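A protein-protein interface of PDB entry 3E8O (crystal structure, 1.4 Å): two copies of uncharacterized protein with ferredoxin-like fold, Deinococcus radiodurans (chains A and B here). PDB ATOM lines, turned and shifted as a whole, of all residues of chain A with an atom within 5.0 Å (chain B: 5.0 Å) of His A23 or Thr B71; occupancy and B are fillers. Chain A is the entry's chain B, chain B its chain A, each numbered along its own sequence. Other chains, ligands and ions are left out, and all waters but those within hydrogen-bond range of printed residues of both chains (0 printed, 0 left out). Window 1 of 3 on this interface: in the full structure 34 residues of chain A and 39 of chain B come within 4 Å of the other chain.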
ATOM      1  N   ILE A  21     -19.570  18.642  18.514  1.00  0.00           N
ATOM      2  CA  ILE A  21     -19.569  19.853  19.321  1.00  0.00           C
ATOM      3  C   ILE A  21     -18.499  19.720  20.373  1.00  0.00           C
ATOM      4  O   ILE A  21     -18.386  18.674  21.040  1.00  0.00           O
ATOM      5  CB  ILE A  21     -20.939  20.020  20.051  1.00  0.00           C
ATOM      6  CG1 ILE A  21     -22.042  20.232  19.039  1.00  0.00           C
ATOM      7  CG2 ILE A  21     -20.874  21.137  21.103  1.00  0.00           C
ATOM      8  CD1 ILE A  21     -23.471  20.239  19.627  1.00  0.00           C
ATOM      9  N   SER A  22     -17.696  20.775  20.508  1.00  0.00           N
ATOM     10  CA  SER A  22     -16.726  20.853  21.607  1.00  0.00           C
ATOM     11  C   SER A  22     -17.154  21.995  22.524  1.00  0.00           C
ATOM     12  O   SER A  22     -17.511  23.075  22.106  1.00  0.00           O
ATOM     13  CB  SER A  22     -15.293  21.048  21.072  1.00  0.00           C
ATOM     14  OG  SER A  22     -14.341  21.000  22.118  1.00  0.00           O
ATOM     15  N   HIS A  23     -17.049  21.710  23.807  1.00  0.00           N
ATOM     16  CA  HIS A  23     -17.353  22.634  24.897  1.00  0.00           C
ATOM     17  C   HIS A  23     -16.137  22.686  25.809  1.00  0.00           C
ATOM     18  O   HIS A  23     -15.751  21.691  26.424  1.00  0.00           O
ATOM     19  CB  HIS A  23     -18.551  22.089  25.670  1.00  0.00           C
ATOM     20  CG  HIS A  23     -18.881  22.864  26.875  1.00  0.00           C
ATOM     21  ND1 HIS A  23     -19.435  24.109  26.795  1.00  0.00           N
ATOM     22  CD2 HIS A  23     -18.689  22.605  28.192  1.00  0.00           C
ATOM     23  CE1 HIS A  23     -19.641  24.566  28.022  1.00  0.00           C
ATOM     24  NE2 HIS A  23     -19.174  23.682  28.880  1.00  0.00           N
ATOM     25  N   GLY A  24     -15.518  23.847  25.837  1.00  0.00           N
ATOM     26  CA  GLY A  24     -14.305  24.069  26.630  1.00  0.00           C
ATOM     27  C   GLY A  24     -14.462  25.219  27.595  1.00  0.00           C
ATOM     28  O   GLY A  24     -15.082  26.238  27.287  1.00  0.00           O
ATOM     29  N   THR A  25     -13.917  25.008  28.781  1.00  0.00           N
ATOM     30  CA  THR A  25     -13.951  26.021  29.857  1.00  0.00           C
ATOM     31  C   THR A  25     -12.563  26.197  30.434  1.00  0.00           C
ATOM     32  O   THR A  25     -11.743  25.256  30.458  1.00  0.00           O
ATOM     33  CB  THR A  25     -14.945  25.627  30.979  1.00  0.00           C
ATOM     34  OG1 THR A  25     -14.631  24.323  31.475  1.00  0.00           O
ATOM     35  CG2 THR A  25     -16.429  25.642  30.473  1.00  0.00           C
ATOM     36  N   LEU A  69     -15.433  30.445  27.819  1.00  0.00           N
ATOM     37  CA  LEU A  69     -16.029  29.314  27.132  1.00  0.00           C
ATOM     38  C   LEU A  69     -15.520  29.297  25.686  1.00  0.00           C
ATOM     39  O   LEU A  69     -15.485  30.335  25.000  1.00  0.00           O
ATOM     40  CB  LEU A  69     -17.569  29.440  27.186  1.00  0.00           C
ATOM     41  CG  LEU A  69     -18.459  28.368  26.512  1.00  0.00           C
ATOM     42  CD1 LEU A  69     -18.404  27.031  27.256  1.00  0.00           C
ATOM     43  CD2 LEU A  69     -19.890  28.771  26.355  1.00  0.00           C
ATOM     44  N   ILE A  70     -15.165  28.103  25.233  1.00  0.00           N
ATOM     45  CA  ILE A  70     -14.745  27.839  23.850  1.00  0.00           C
ATOM     46  C   ILE A  70     -15.792  26.907  23.265  1.00  0.00           C
ATOM     47  O   ILE A  70     -15.947  25.779  23.693  1.00  0.00           O
ATOM     48  CB  ILE A  70     -13.374  27.234  23.732  1.00  0.00           C
ATOM     49  CG1 ILE A  70     -12.343  28.003  24.549  1.00  0.00           C
ATOM     50  CG2 ILE A  70     -12.952  27.163  22.219  1.00  0.00           C
ATOM     51  CD1 ILE A  70     -10.960  27.345  24.523  1.00  0.00           C
ATOM     52  N   THR A  71     -16.553  27.434  22.326  1.00  0.00           N
ATOM     53  CA  THR A  71     -17.654  26.696  21.690  1.00  0.00           C
ATOM     54  C   THR A  71     -17.239  26.386  20.267  1.00  0.00           C
ATOM     55  O   THR A  71     -17.009  27.310  19.477  1.00  0.00           O
ATOM     56  CB  THR A  71     -18.940  27.561  21.684  1.00  0.00           C
ATOM     57  OG1 THR A  71     -19.280  27.896  23.027  1.00  0.00           O
ATOM     58  CG2 THR A  71     -20.105  26.826  20.998  1.00  0.00           C
ATOM     59  N   LYS A 105     -10.592  22.539  30.585  1.00  0.00           N
ATOM     60  CA  LYS A 105     -11.377  21.304  30.405  1.00  0.00           C
ATOM     61  C   LYS A 105     -12.081  21.382  29.060  1.00  0.00           C
ATOM     62  O   LYS A 105     -12.739  22.357  28.763  1.00  0.00           O
ATOM     63  CB  LYS A 105     -12.401  21.101  31.533  1.00  0.00           C
ATOM     64  CG  LYS A 105     -13.157  19.812  31.445  1.00  0.00           C
ATOM     65  CD  LYS A 105     -14.035  19.619  32.672  1.00  0.00           C
ATOM     66  CE  LYS A 105     -14.669  18.221  32.636  1.00  0.00           C
ATOM     67  NZ  LYS A 105     -13.631  17.147  32.481  1.00  0.00           N
ATOM     68  N   ILE A 106     -11.888  20.353  28.250  1.00  0.00           N
ATOM     69  CA  ILE A 106     -12.525  20.281  26.951  1.00  0.00           C
ATOM     70  C   ILE A 106     -13.200  18.939  26.797  1.00  0.00           C
ATOM     71  O   ILE A 106     -12.573  17.902  27.025  1.00  0.00           O
ATOM     72  CB  ILE A 106     -11.536  20.489  25.809  1.00  0.00           C
ATOM     73  CG1 ILE A 106     -10.753  21.790  26.000  1.00  0.00           C
ATOM     74  CG2 ILE A 106     -12.268  20.400  24.479  1.00  0.00           C
ATOM     75  CD1 ILE A 106      -9.775  22.020  24.888  1.00  0.00           C
ATOM     76  N   THR A 107     -14.488  19.006  26.473  1.00  0.00           N
ATOM     77  CA  THR A 107     -15.325  17.820  26.272  1.00  0.00           C
ATOM     78  C   THR A 107     -16.021  17.957  24.933  1.00  0.00           C
ATOM     79  O   THR A 107     -16.601  19.000  24.613  1.00  0.00           O
ATOM     80  CB  THR A 107     -16.362  17.658  27.411  1.00  0.00           C
ATOM     81  OG1 THR A 107     -15.711  17.826  28.668  1.00  0.00           O
ATOM     82  CG2 THR A 107     -17.017  16.305  27.381  1.00  0.00           C
ATOM     83  N   ALA A 108     -15.989  16.889  24.151  1.00  0.00           N
ATOM     84  CA  ALA A 108     -16.640  16.870  22.856  1.00  0.00           C
ATOM     85  C   ALA A 108     -17.726  15.838  22.844  1.00  0.00           C
ATOM     86  O   ALA A 108     -17.741  14.903  23.646  1.00  0.00           O
ATOM     87  CB  ALA A 108     -15.624  16.616  21.686  1.00  0.00           C
ATOM     88  N   TYR A 109     -18.660  16.078  21.943  1.00  0.00           N
ATOM     89  CA  TYR A 109     -19.838  15.210  21.788  1.00  0.00           C
ATOM     90  C   TYR A 109     -20.243  15.131  20.333  1.00  0.00           C
ATOM     91  O   TYR A 109     -20.312  16.152  19.640  1.00  0.00           O
ATOM     92  CB  TYR A 109     -21.048  15.807  22.533  1.00  0.00           C
ATOM     93  CG  TYR A 109     -20.810  16.211  23.964  1.00  0.00           C
ATOM     94  CD1 TYR A 109     -20.309  17.476  24.282  1.00  0.00           C
ATOM     95  CD2 TYR A 109     -21.077  15.364  24.988  1.00  0.00           C
ATOM     96  CE1 TYR A 109     -20.093  17.841  25.573  1.00  0.00           C
ATOM     97  CE2 TYR A 109     -20.909  15.753  26.284  1.00  0.00           C
ATOM     98  CZ  TYR A 109     -20.370  16.969  26.564  1.00  0.00           C
ATOM     99  OH  TYR A 109     -20.185  17.327  27.904  1.00  0.00           O
ATOM    100  N   SER B  22     -28.022  22.534  23.974  1.00  0.00           N
ATOM    101  CA  SER B  22     -28.653  23.700  23.300  1.00  0.00           C
ATOM    102  C   SER B  22     -27.616  24.791  23.092  1.00  0.00           C
ATOM    103  O   SER B  22     -26.801  25.077  23.989  1.00  0.00           O
ATOM    104  CB  SER B  22     -29.764  24.271  24.183  1.00  0.00           C
ATOM    105  OG  SER B  22     -30.611  25.188  23.505  1.00  0.00           O
ATOM    106  N   LEU B  55     -26.349  22.065  32.882  1.00  0.00           N
ATOM    107  CA  LEU B  55     -25.492  23.225  32.608  1.00  0.00           C
ATOM    108  C   LEU B  55     -26.343  24.324  31.991  1.00  0.00           C
ATOM    109  O   LEU B  55     -27.169  24.065  31.127  1.00  0.00           O
ATOM    110  CB  LEU B  55     -24.401  22.886  31.600  1.00  0.00           C
ATOM    111  CG  LEU B  55     -23.337  23.969  31.368  1.00  0.00           C
ATOM    112  CD1 LEU B  55     -22.449  24.172  32.593  1.00  0.00           C
ATOM    113  CD2 LEU B  55     -22.512  23.600  30.138  1.00  0.00           C
ATOM    114  N   TYR B  56     -26.130  25.541  32.431  1.00  0.00           N
ATOM    115  CA  TYR B  56     -26.768  26.727  31.813  1.00  0.00           C
ATOM    116  C   TYR B  56     -25.834  27.904  32.016  1.00  0.00           C
ATOM    117  O   TYR B  56     -25.669  28.407  33.113  1.00  0.00           O
ATOM    118  CB  TYR B  56     -28.140  27.004  32.420  1.00  0.00           C
ATOM    119  CG  TYR B  56     -29.004  27.909  31.576  1.00  0.00           C
ATOM    120  CD1 TYR B  56     -28.817  29.256  31.558  1.00  0.00           C
ATOM    121  CD2 TYR B  56     -30.084  27.410  30.872  1.00  0.00           C
ATOM    122  CE1 TYR B  56     -29.612  30.085  30.793  1.00  0.00           C
ATOM    123  CE2 TYR B  56     -30.891  28.220  30.134  1.00  0.00           C
ATOM    124  CZ  TYR B  56     -30.670  29.570  30.097  1.00  0.00           C
ATOM    125  OH  TYR B  56     -31.430  30.457  29.373  1.00  0.00           O
ATOM    126  N   LEU B  57     -25.181  28.288  30.941  1.00  0.00           N
ATOM    127  CA  LEU B  57     -24.231  29.387  30.928  1.00  0.00           C
ATOM    128  C   LEU B  57     -24.660  30.469  29.939  1.00  0.00           C
ATOM    129  O   LEU B  57     -25.125  30.202  28.831  1.00  0.00           O
ATOM    130  CB  LEU B  57     -22.844  28.902  30.477  1.00  0.00           C
ATOM    131  CG  LEU B  57     -22.165  27.836  31.292  1.00  0.00           C
ATOM    132  CD1 LEU B  57     -20.891  27.336  30.576  1.00  0.00           C
ATOM    133  CD2 LEU B  57     -21.868  28.327  32.682  1.00  0.00           C
ATOM    134  N   LEU B  69     -24.227  34.409  24.033  1.00  0.00           N
ATOM    135  CA  LEU B  69     -24.412  32.982  23.851  1.00  0.00           C
ATOM    136  C   LEU B  69     -25.113  32.396  25.075  1.00  0.00           C
ATOM    137  O   LEU B  69     -24.822  32.777  26.214  1.00  0.00           O
ATOM    138  CB  LEU B  69     -23.034  32.300  23.647  1.00  0.00           C
ATOM    139  CG  LEU B  69     -22.888  30.802  23.342  1.00  0.00           C
ATOM    140  CD1 LEU B  69     -23.524  30.413  22.000  1.00  0.00           C
ATOM    141  CD2 LEU B  69     -21.388  30.384  23.355  1.00  0.00           C
ATOM    142  N   ILE B  70     -25.998  31.449  24.817  1.00  0.00           N
ATOM    143  CA  ILE B  70     -26.690  30.687  25.830  1.00  0.00           C
ATOM    144  C   ILE B  70     -26.333  29.223  25.562  1.00  0.00           C
ATOM    145  O   ILE B  70     -26.678  28.656  24.513  1.00  0.00           O
ATOM    146  CB  ILE B  70     -28.216  30.866  25.844  1.00  0.00           C
ATOM    147  CG1 ILE B  70     -28.659  32.336  25.866  1.00  0.00           C
ATOM    148  CG2 ILE B  70     -28.806  30.109  27.007  1.00  0.00           C
ATOM    149  CD1 ILE B  70     -30.149  32.551  25.799  1.00  0.00           C
ATOM    150  N   THR B  71     -25.646  28.605  26.516  1.00  0.00           N
ATOM    151  CA  THR B  71     -25.151  27.231  26.433  1.00  0.00           C
ATOM    152  C   THR B  71     -25.856  26.391  27.476  1.00  0.00           C
ATOM    153  O   THR B  71     -25.811  26.701  28.657  1.00  0.00           O
ATOM    154  CB  THR B  71     -23.644  27.214  26.652  1.00  0.00           C
ATOM    155  OG1 THR B  71     -23.030  28.084  25.705  1.00  0.00           O
ATOM    156  CG2 THR B  71     -23.044  25.801  26.577  1.00  0.00           C
ATOM    157  N   GLU B  72     -26.539  25.339  27.023  1.00  0.00           N
ATOM    158  CA  GLU B  72     -27.304  24.521  27.968  1.00  0.00           C
ATOM    159  C   GLU B  72     -27.087  23.044  27.727  1.00  0.00           C
ATOM    160  O   GLU B  72     -27.012  22.614  26.599  1.00  0.00           O
ATOM    161  CB  GLU B  72     -28.839  24.780  27.839  1.00  0.00           C
ATOM    162  CG  GLU B  72     -29.242  26.214  27.617  1.00  0.00           C
ATOM    163  CD  GLU B  72     -30.696  26.464  27.326  1.00  0.00           C
ATOM    164  OE1 GLU B  72     -31.553  25.693  27.823  1.00  0.00           O
ATOM    165  OE2 GLU B  72     -30.995  27.484  26.635  1.00  0.00           O
ATOM    166  N   HIS B  73     -27.036  22.292  28.821  1.00  0.00           N
ATOM    167  CA  HIS B  73     -27.034  20.827  28.771  1.00  0.00           C
ATOM    168  C   HIS B  73     -28.191  20.335  29.614  1.00  0.00           C
ATOM    169  O   HIS B  73     -28.346  20.737  30.754  1.00  0.00           O
ATOM    170  CB  HIS B  73     -25.740  20.205  29.316  1.00  0.00           C
ATOM    171  CG  HIS B  73     -24.524  20.546  28.542  1.00  0.00           C
ATOM    172  ND1 HIS B  73     -23.278  20.131  28.957  1.00  0.00           N
ATOM    173  CD2 HIS B  73     -24.336  21.273  27.411  1.00  0.00           C
ATOM    174  CE1 HIS B  73     -22.379  20.564  28.086  1.00  0.00           C
ATOM    175  NE2 HIS B  73     -22.990  21.267  27.148  1.00  0.00           N
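Hydrophobic or aromatic side chains of chain B that line the printed part of chain A: Leu B55, Leu B57, Leu B69 and His B73.
Of the 13 printed residues of chain A, 4 touch a printed residue of chain B.
Hydrophobic or aromatic side chains of chain A within 4 Å of the printed part of chain B: His A23, Leu A69 and Tyr A109.
Among the printed residues, no Asp or Glu carboxylate lies within 4 Å of a Lys or Arg side-chain nitrogen of the other chain.
The backbone carbonyl oxygen (O) of Leu B55 is in hydrogen-bond range of the backbone NH (N) of His B73, 2.9 Å away.
O of Thr B71 sits at hydrogen-bond distance from N of Leu B57, 2.9 Å away.
O of Ile A21 sits at hydrogen-bond distance from N of Tyr A109, 2.8 Å away.
O of Thr A107 is in hydrogen-bond range of N of His A23 (2.9 Å).
Among the printed residues, merely in contact across the chains: His A23 with Leu B55, His A23 with Leu B57, His A23 with Thr B71, Leu A69 with Leu B69, Leu A69 with Thr B71, Thr A71 with Leu B69 and Tyr A109 with His B73.
Of the printed residues of chain B, Leu A69 touches Leu B69 (3.7 Å) and Thr B71 (3.3 Å).
Of the printed residues of chain B, Thr A71 touches Leu B69.
Of the printed residues of chain A, Leu B55 touches His A23.
Of the printed residues of chain A, Leu B57 touches His A23.
The nearest printed residue of chain B that does not touch Tyr A109 is Leu B55 (7.1 Å).
Leu B69 touches its own counterpart, Leu A69.
Leu A69 touches Thr B71, and with the chains exchanged Thr A71 touches Leu B69.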
